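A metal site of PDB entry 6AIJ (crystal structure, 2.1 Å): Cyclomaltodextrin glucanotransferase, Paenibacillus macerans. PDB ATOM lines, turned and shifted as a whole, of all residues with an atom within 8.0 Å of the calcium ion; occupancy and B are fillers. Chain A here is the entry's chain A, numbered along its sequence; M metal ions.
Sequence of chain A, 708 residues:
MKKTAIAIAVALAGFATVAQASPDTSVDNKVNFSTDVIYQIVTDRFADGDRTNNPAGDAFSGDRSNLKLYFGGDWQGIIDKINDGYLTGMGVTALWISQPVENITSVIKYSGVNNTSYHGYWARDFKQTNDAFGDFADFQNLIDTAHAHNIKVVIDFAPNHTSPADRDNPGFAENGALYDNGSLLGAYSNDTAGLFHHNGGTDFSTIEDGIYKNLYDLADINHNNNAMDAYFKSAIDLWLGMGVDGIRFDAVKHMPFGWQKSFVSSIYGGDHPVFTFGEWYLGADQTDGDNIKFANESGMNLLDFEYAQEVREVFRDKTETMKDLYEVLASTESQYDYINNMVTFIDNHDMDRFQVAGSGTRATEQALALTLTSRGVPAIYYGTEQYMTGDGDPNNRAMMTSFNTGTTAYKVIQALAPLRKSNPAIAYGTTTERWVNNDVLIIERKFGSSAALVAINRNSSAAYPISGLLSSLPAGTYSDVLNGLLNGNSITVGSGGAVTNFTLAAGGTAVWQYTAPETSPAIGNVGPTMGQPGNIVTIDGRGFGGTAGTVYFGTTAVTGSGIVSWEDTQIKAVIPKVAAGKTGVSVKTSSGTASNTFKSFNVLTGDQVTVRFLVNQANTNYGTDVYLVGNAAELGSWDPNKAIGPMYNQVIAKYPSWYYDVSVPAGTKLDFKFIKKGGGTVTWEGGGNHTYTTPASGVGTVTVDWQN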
ATOM      1  N   THR A  43     -26.887  18.007  -4.189  1.00  0.00           N
ATOM      2  CA  THR A  43     -27.208  18.521  -5.509  1.00  0.00           C
ATOM      3  C   THR A  43     -27.549  17.422  -6.504  1.00  0.00           C
ATOM      4  O   THR A  43     -28.559  17.515  -7.234  1.00  0.00           O
ATOM      5  CB  THR A  43     -26.027  19.350  -6.031  1.00  0.00           C
ATOM      6  OG1 THR A  43     -25.763  20.429  -5.113  1.00  0.00           O
ATOM      7  CG2 THR A  43     -26.330  19.947  -7.423  1.00  0.00           C
ATOM      8  N   ASP A  44     -26.729  16.363  -6.578  1.00  0.00           N
ATOM      9  CA  ASP A  44     -26.953  15.297  -7.564  1.00  0.00           C
ATOM     10  C   ASP A  44     -28.272  14.546  -7.346  1.00  0.00           C
ATOM     11  O   ASP A  44     -28.752  13.866  -8.270  1.00  0.00           O
ATOM     12  CB  ASP A  44     -25.795  14.298  -7.528  1.00  0.00           C
ATOM     13  CG  ASP A  44     -25.910  13.238  -8.615  1.00  0.00           C
ATOM     14  OD1 ASP A  44     -25.853  13.590  -9.805  1.00  0.00           O
ATOM     15  OD2 ASP A  44     -26.040  12.048  -8.258  1.00  0.00           O
ATOM     16  N   ALA A  47     -32.817  17.386  -8.268  1.00  0.00           N
ATOM     17  CA  ALA A  47     -33.626  17.587  -9.477  1.00  0.00           C
ATOM     18  C   ALA A  47     -32.717  17.723 -10.692  1.00  0.00           C
ATOM     19  O   ALA A  47     -31.865  18.615 -10.718  1.00  0.00           O
ATOM     20  CB  ALA A  47     -34.518  18.847  -9.353  1.00  0.00           C
ATOM     21  N   ASP A  48     -32.907  16.873 -11.698  1.00  0.00           N
ATOM     22  CA  ASP A  48     -32.126  16.944 -12.929  1.00  0.00           C
ATOM     23  C   ASP A  48     -32.835  17.895 -13.898  1.00  0.00           C
ATOM     24  O   ASP A  48     -33.749  17.498 -14.617  1.00  0.00           O
ATOM     25  CB  ASP A  48     -31.948  15.556 -13.537  1.00  0.00           C
ATOM     26  CG  ASP A  48     -31.053  15.567 -14.786  1.00  0.00           C
ATOM     27  OD1 ASP A  48     -30.616  16.659 -15.214  1.00  0.00           O
ATOM     28  OD2 ASP A  48     -30.805  14.474 -15.344  1.00  0.00           O
ATOM     29  N   GLY A  49     -32.396  19.156 -13.901  1.00  0.00           N
ATOM     30  CA  GLY A  49     -32.916  20.172 -14.778  1.00  0.00           C
ATOM     31  C   GLY A  49     -32.197  20.333 -16.101  1.00  0.00           C
ATOM     32  O   GLY A  49     -32.588  21.168 -16.916  1.00  0.00           O
ATOM     33  N   ASP A  50     -31.134  19.553 -16.336  1.00  0.00           N
ATOM     34  CA  ASP A  50     -30.377  19.642 -17.581  1.00  0.00           C
ATOM     35  C   ASP A  50     -29.707  18.289 -17.790  1.00  0.00           C
ATOM     36  O   ASP A  50     -28.688  17.990 -17.162  1.00  0.00           O
ATOM     37  CB  ASP A  50     -29.367  20.787 -17.500  1.00  0.00           C
ATOM     38  CG  ASP A  50     -28.471  20.888 -18.731  1.00  0.00           C
ATOM     39  OD1 ASP A  50     -28.740  20.228 -19.747  1.00  0.00           O
ATOM     40  OD2 ASP A  50     -27.493  21.655 -18.662  1.00  0.00           O
ATOM     41  N   ARG A  51     -30.278  17.464 -18.669  1.00  0.00           N
ATOM     42  CA  ARG A  51     -29.692  16.161 -18.949  1.00  0.00           C
ATOM     43  C   ARG A  51     -28.424  16.227 -19.785  1.00  0.00           C
ATOM     44  O   ARG A  51     -27.705  15.220 -19.850  1.00  0.00           O
ATOM     45  CB  ARG A  51     -30.724  15.272 -19.617  1.00  0.00           C
ATOM     46  CG  ARG A  51     -31.704  14.666 -18.632  1.00  0.00           C
ATOM     47  CD  ARG A  51     -33.112  15.076 -18.959  1.00  0.00           C
ATOM     48  NE  ARG A  51     -33.345  16.504 -18.731  1.00  0.00           N
ATOM     49  CZ  ARG A  51     -34.325  17.176 -19.301  1.00  0.00           C
ATOM     50  NH1 ARG A  51     -35.155  16.554 -20.130  1.00  0.00           N
ATOM     51  NH2 ARG A  51     -34.472  18.481 -19.050  1.00  0.00           N
ATOM     52  N   THR A  52     -28.100  17.360 -20.406  1.00  0.00           N
ATOM     53  CA  THR A  52     -26.899  17.448 -21.238  1.00  0.00           C
ATOM     54  C   THR A  52     -25.611  17.524 -20.432  1.00  0.00           C
ATOM     55  O   THR A  52     -24.538  17.237 -20.974  1.00  0.00           O
ATOM     56  CB  THR A  52     -26.958  18.643 -22.188  1.00  0.00           C
ATOM     57  OG1 THR A  52     -26.674  19.853 -21.460  1.00  0.00           O
ATOM     58  CG2 THR A  52     -28.302  18.737 -22.879  1.00  0.00           C
ATOM     59  N   ASN A  53     -25.668  17.914 -19.155  1.00  0.00           N
ATOM     60  CA  ASN A  53     -24.494  17.870 -18.300  1.00  0.00           C
ATOM     61  C   ASN A  53     -24.419  16.584 -17.480  1.00  0.00           C
ATOM     62  O   ASN A  53     -23.621  16.497 -16.537  1.00  0.00           O
ATOM     63  CB  ASN A  53     -24.453  19.087 -17.375  1.00  0.00           C
ATOM     64  CG  ASN A  53     -25.623  19.137 -16.386  1.00  0.00           C
ATOM     65  OD1 ASN A  53     -26.196  18.116 -16.019  1.00  0.00           O
ATOM     66  ND2 ASN A  53     -25.955  20.329 -15.932  1.00  0.00           N
ATOM     67  N   ASN A  54     -25.237  15.598 -17.818  1.00  0.00           N
ATOM     68  CA  ASN A  54     -25.241  14.333 -17.091  1.00  0.00           C
ATOM     69  C   ASN A  54     -23.984  13.540 -17.412  1.00  0.00           C
ATOM     70  O   ASN A  54     -23.697  13.312 -18.590  1.00  0.00           O
ATOM     71  CB  ASN A  54     -26.481  13.517 -17.454  1.00  0.00           C
ATOM     72  CG  ASN A  54     -27.692  13.941 -16.680  1.00  0.00           C
ATOM     73  OD1 ASN A  54     -27.669  14.956 -15.986  1.00  0.00           O
ATOM     74  ND2 ASN A  54     -28.763  13.170 -16.785  1.00  0.00           N
ATOM     75  N   PRO A  55     -23.220  13.121 -16.401  1.00  0.00           N
ATOM     76  CA  PRO A  55     -22.083  12.208 -16.660  1.00  0.00           C
ATOM     77  C   PRO A  55     -22.524  10.954 -17.396  1.00  0.00           C
ATOM     78  O   PRO A  55     -23.653  10.489 -17.255  1.00  0.00           O
ATOM     79  CB  PRO A  55     -21.584  11.882 -15.253  1.00  0.00           C
ATOM     80  CG  PRO A  55     -22.034  13.048 -14.403  1.00  0.00           C
ATOM     81  CD  PRO A  55     -23.331  13.510 -14.992  1.00  0.00           C
ATOM     82  N   PHE A  60     -22.499   7.102 -14.286  1.00  0.00           N
ATOM     83  CA  PHE A  60     -23.901   7.457 -14.228  1.00  0.00           C
ATOM     84  C   PHE A  60     -24.747   6.216 -13.959  1.00  0.00           C
ATOM     85  O   PHE A  60     -24.484   5.143 -14.516  1.00  0.00           O
ATOM     86  CB  PHE A  60     -24.343   8.119 -15.543  1.00  0.00           C
ATOM     87  CG  PHE A  60     -25.704   8.770 -15.485  1.00  0.00           C
ATOM     88  CD1 PHE A  60     -25.837  10.092 -15.055  1.00  0.00           C
ATOM     89  CD2 PHE A  60     -26.843   8.078 -15.863  1.00  0.00           C
ATOM     90  CE1 PHE A  60     -27.081  10.691 -14.996  1.00  0.00           C
ATOM     91  CE2 PHE A  60     -28.089   8.673 -15.814  1.00  0.00           C
ATOM     92  CZ  PHE A  60     -28.204   9.981 -15.382  1.00  0.00           C
ATOM     93  N   TYR A  70     -23.362   9.145 -10.140  1.00  0.00           N
ATOM     94  CA  TYR A  70     -24.113  10.350 -10.448  1.00  0.00           C
ATOM     95  C   TYR A  70     -25.502   9.995 -10.932  1.00  0.00           C
ATOM     96  O   TYR A  70     -25.650   9.144 -11.825  1.00  0.00           O
ATOM     97  CB  TYR A  70     -23.395  11.163 -11.515  1.00  0.00           C
ATOM     98  CG  TYR A  70     -22.268  12.049 -11.029  1.00  0.00           C
ATOM     99  CD1 TYR A  70     -20.953  11.580 -10.990  1.00  0.00           C
ATOM    100  CD2 TYR A  70     -22.511  13.359 -10.628  1.00  0.00           C
ATOM    101  CE1 TYR A  70     -19.920  12.394 -10.565  1.00  0.00           C
ATOM    102  CE2 TYR A  70     -21.478  14.172 -10.204  1.00  0.00           C
ATOM    103  CZ  TYR A  70     -20.175  13.691 -10.180  1.00  0.00           C
ATOM    104  OH  TYR A  70     -19.126  14.488  -9.762  1.00  0.00           O
ATOM    105  N   PHE A  71     -26.513  10.639 -10.353  1.00  0.00           N
ATOM    106  CA  PHE A  71     -27.901  10.503 -10.785  1.00  0.00           C
ATOM    107  C   PHE A  71     -28.345  11.601 -11.766  1.00  0.00           C
ATOM    108  O   PHE A  71     -29.291  11.378 -12.519  1.00  0.00           O
ATOM    109  CB  PHE A  71     -28.843  10.536  -9.579  1.00  0.00           C
ATOM    110  CG  PHE A  71     -28.921   9.243  -8.805  1.00  0.00           C
ATOM    111  CD1 PHE A  71     -28.082   8.181  -9.078  1.00  0.00           C
ATOM    112  CD2 PHE A  71     -29.867   9.093  -7.796  1.00  0.00           C
ATOM    113  CE1 PHE A  71     -28.180   6.993  -8.355  1.00  0.00           C
ATOM    114  CE2 PHE A  71     -29.961   7.918  -7.079  1.00  0.00           C
ATOM    115  CZ  PHE A  71     -29.126   6.864  -7.355  1.00  0.00           C
ATOM    116  N   GLY A  72     -27.728  12.785 -11.726  1.00  0.00           N
ATOM    117  CA  GLY A  72     -28.042  13.846 -12.682  1.00  0.00           C
ATOM    118  C   GLY A  72     -28.526  15.166 -12.077  1.00  0.00           C
ATOM    119  O   GLY A  72     -28.688  16.138 -12.826  1.00  0.00           O
ATOM    120  N   GLY A  73     -28.782  15.247 -10.776  1.00  0.00           N
ATOM    121  CA  GLY A  73     -29.276  16.499 -10.218  1.00  0.00           C
ATOM    122  C   GLY A  73     -28.256  17.617 -10.358  1.00  0.00           C
ATOM    123  O   GLY A  73     -27.050  17.396 -10.281  1.00  0.00           O
ATOM    124  N   ASP A  74     -28.752  18.837 -10.587  1.00  0.00           N
ATOM    125  CA  ASP A  74     -27.859  19.920 -10.953  1.00  0.00           C
ATOM    126  C   ASP A  74     -28.452  21.253 -10.530  1.00  0.00           C
ATOM    127  O   ASP A  74     -29.589  21.334 -10.034  1.00  0.00           O
ATOM    128  CB  ASP A  74     -27.567  19.904 -12.452  1.00  0.00           C
ATOM    129  CG  ASP A  74     -28.840  19.828 -13.283  1.00  0.00           C
ATOM    130  OD1 ASP A  74     -29.837  20.481 -12.930  1.00  0.00           O
ATOM    131  OD2 ASP A  74     -28.835  19.119 -14.307  1.00  0.00           O
ATOM    132  N   TRP A  75     -27.668  22.323 -10.739  1.00  0.00           N
ATOM    133  CA  TRP A  75     -28.113  23.651 -10.330  1.00  0.00           C
ATOM    134  C   TRP A  75     -29.344  24.092 -11.110  1.00  0.00           C
ATOM    135  O   TRP A  75     -30.227  24.743 -10.547  1.00  0.00           O
ATOM    136  CB  TRP A  75     -26.966  24.660 -10.481  1.00  0.00           C
ATOM    137  CG  TRP A  75     -25.807  24.341  -9.563  1.00  0.00           C
ATOM    138  CD1 TRP A  75     -25.883  23.768  -8.320  1.00  0.00           C
ATOM    139  CD2 TRP A  75     -24.408  24.539  -9.830  1.00  0.00           C
ATOM    140  NE1 TRP A  75     -24.615  23.602  -7.795  1.00  0.00           N
ATOM    141  CE2 TRP A  75     -23.693  24.069  -8.700  1.00  0.00           C
ATOM    142  CE3 TRP A  75     -23.691  25.062 -10.907  1.00  0.00           C
ATOM    143  CZ2 TRP A  75     -22.299  24.120  -8.629  1.00  0.00           C
ATOM    144  CZ3 TRP A  75     -22.297  25.112 -10.836  1.00  0.00           C
ATOM    145  CH2 TRP A  75     -21.621  24.636  -9.697  1.00  0.00           C
ATOM    146  N   GLN A  76     -29.455  23.715 -12.383  1.00  0.00           N
ATOM    147  CA  GLN A  76     -30.649  24.064 -13.142  1.00  0.00           C
ATOM    148  C   GLN A  76     -31.912  23.529 -12.485  1.00  0.00           C
ATOM    149  O   GLN A  76     -32.944  24.207 -12.444  1.00  0.00           O
ATOM    150  CB  GLN A  76     -30.545  23.546 -14.572  1.00  0.00           C
ATOM    151  CG  GLN A  76     -31.701  24.047 -15.446  1.00  0.00           C
ATOM    152  CD  GLN A  76     -31.662  25.558 -15.600  1.00  0.00           C
ATOM    153  OE1 GLN A  76     -30.733  26.114 -16.193  1.00  0.00           O
ATOM    154  NE2 GLN A  76     -32.674  26.231 -15.077  1.00  0.00           N
ATOM    155  N   GLY A  77     -31.845  22.303 -11.953  1.00  0.00           N
ATOM    156  CA  GLY A  77     -32.984  21.730 -11.260  1.00  0.00           C
ATOM    157  C   GLY A  77     -33.361  22.503 -10.006  1.00  0.00           C
ATOM    158  O   GLY A  77     -34.534  22.710  -9.731  1.00  0.00           O
ATOM    159  N   ASP A 131     -18.700  20.269 -13.465  1.00  0.00           N
ATOM    160  CA  ASP A 131     -19.541  20.462 -14.642  1.00  0.00           C
ATOM    161  C   ASP A 131     -20.817  19.616 -14.612  1.00  0.00           C
ATOM    162  O   ASP A 131     -21.750  19.904 -15.394  1.00  0.00           O
ATOM    163  CB  ASP A 131     -18.764  20.146 -15.919  1.00  0.00           C
ATOM    164  CG  ASP A 131     -17.535  21.026 -16.098  1.00  0.00           C
ATOM    165  OD1 ASP A 131     -17.438  22.118 -15.483  1.00  0.00           O
ATOM    166  OD2 ASP A 131     -16.651  20.608 -16.869  1.00  0.00           O
ATOM    167  N   ALA A 132     -20.883  18.575 -13.780  1.00  0.00           N
ATOM    168  CA  ALA A 132     -22.144  17.868 -13.602  1.00  0.00           C
ATOM    169  C   ALA A 132     -23.214  18.784 -13.037  1.00  0.00           C
ATOM    170  O   ALA A 132     -24.385  18.710 -13.437  1.00  0.00           O
ATOM    171  CB  ALA A 132     -21.954  16.666 -12.685  1.00  0.00           C
ATOM    172  N   PHE A 133     -22.841  19.655 -12.107  1.00  0.00           N
ATOM    173  CA  PHE A 133     -23.824  20.558 -11.509  1.00  0.00           C
ATOM    174  C   PHE A 133     -24.139  21.740 -12.417  1.00  0.00           C
ATOM    175  O   PHE A 133     -25.275  22.247 -12.395  1.00  0.00           O
ATOM    176  CB  PHE A 133     -23.294  21.062 -10.169  1.00  0.00           C
ATOM    177  CG  PHE A 133     -22.999  19.965  -9.183  1.00  0.00           C
ATOM    178  CD1 PHE A 133     -23.585  18.709  -9.319  1.00  0.00           C
ATOM    179  CD2 PHE A 133     -22.156  20.192  -8.115  1.00  0.00           C
ATOM    180  CE1 PHE A 133     -23.321  17.704  -8.399  1.00  0.00           C
ATOM    181  CE2 PHE A 133     -21.882  19.195  -7.189  1.00  0.00           C
ATOM    182  CZ  PHE A 133     -22.464  17.951  -7.331  1.00  0.00           C
ATOM    183  N   GLY A 134     -23.180  22.191 -13.213  1.00  0.00           N
ATOM    184  CA  GLY A 134     -23.370  23.283 -14.139  1.00  0.00           C
ATOM    185  C   GLY A 134     -22.033  23.966 -14.420  1.00  0.00           C
ATOM    186  O   GLY A 134     -20.995  23.603 -13.879  1.00  0.00           O
HETATM  187 CA    CA M   1     -28.057  17.084 -14.988  1.00  0.00          CA
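The calcium ion is bound by OD2 of Asp 74 (2.3 Å), OD1 of Asn 53 (2.4 Å), OD1 of Asn 54 (2.4 Å), O of Asp 50 (2.4 Å), O of Gly 72 (2.4 Å) and OD1 of Asp 48 (2.6 Å). The calcium ion has six donor atoms within binding distance.
OD1 of Asp 50 is in hydrogen-bond range of OG1 of Thr 52, 2.7 Å away. O of Ala 132 lies close to ND2 of Asn 53, 3.4 Å away. The side-chain carboxylate (OD1) of Asp 44 is in hydrogen-bond range of the backbone NH (N) of Gly 72, 2.8 Å away. The backbone NH (N) of Gln 76 lies close to the side-chain carboxylate (OD1) of Asp 74 (3.3 Å). N of Gly 77 sits at hydrogen-bond distance from OD1 of Asp 74, at 2.9 Å. The side-chain carboxylate (OD1) of Asp 74 lies within hydrogen-bond range of the backbone NH (N) of Gly 49 (3.0 Å). The backbone NH of Asp 74 lies within hydrogen-bond range of the backbone carbonyl oxygen of Ala 47 (3.1 Å).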
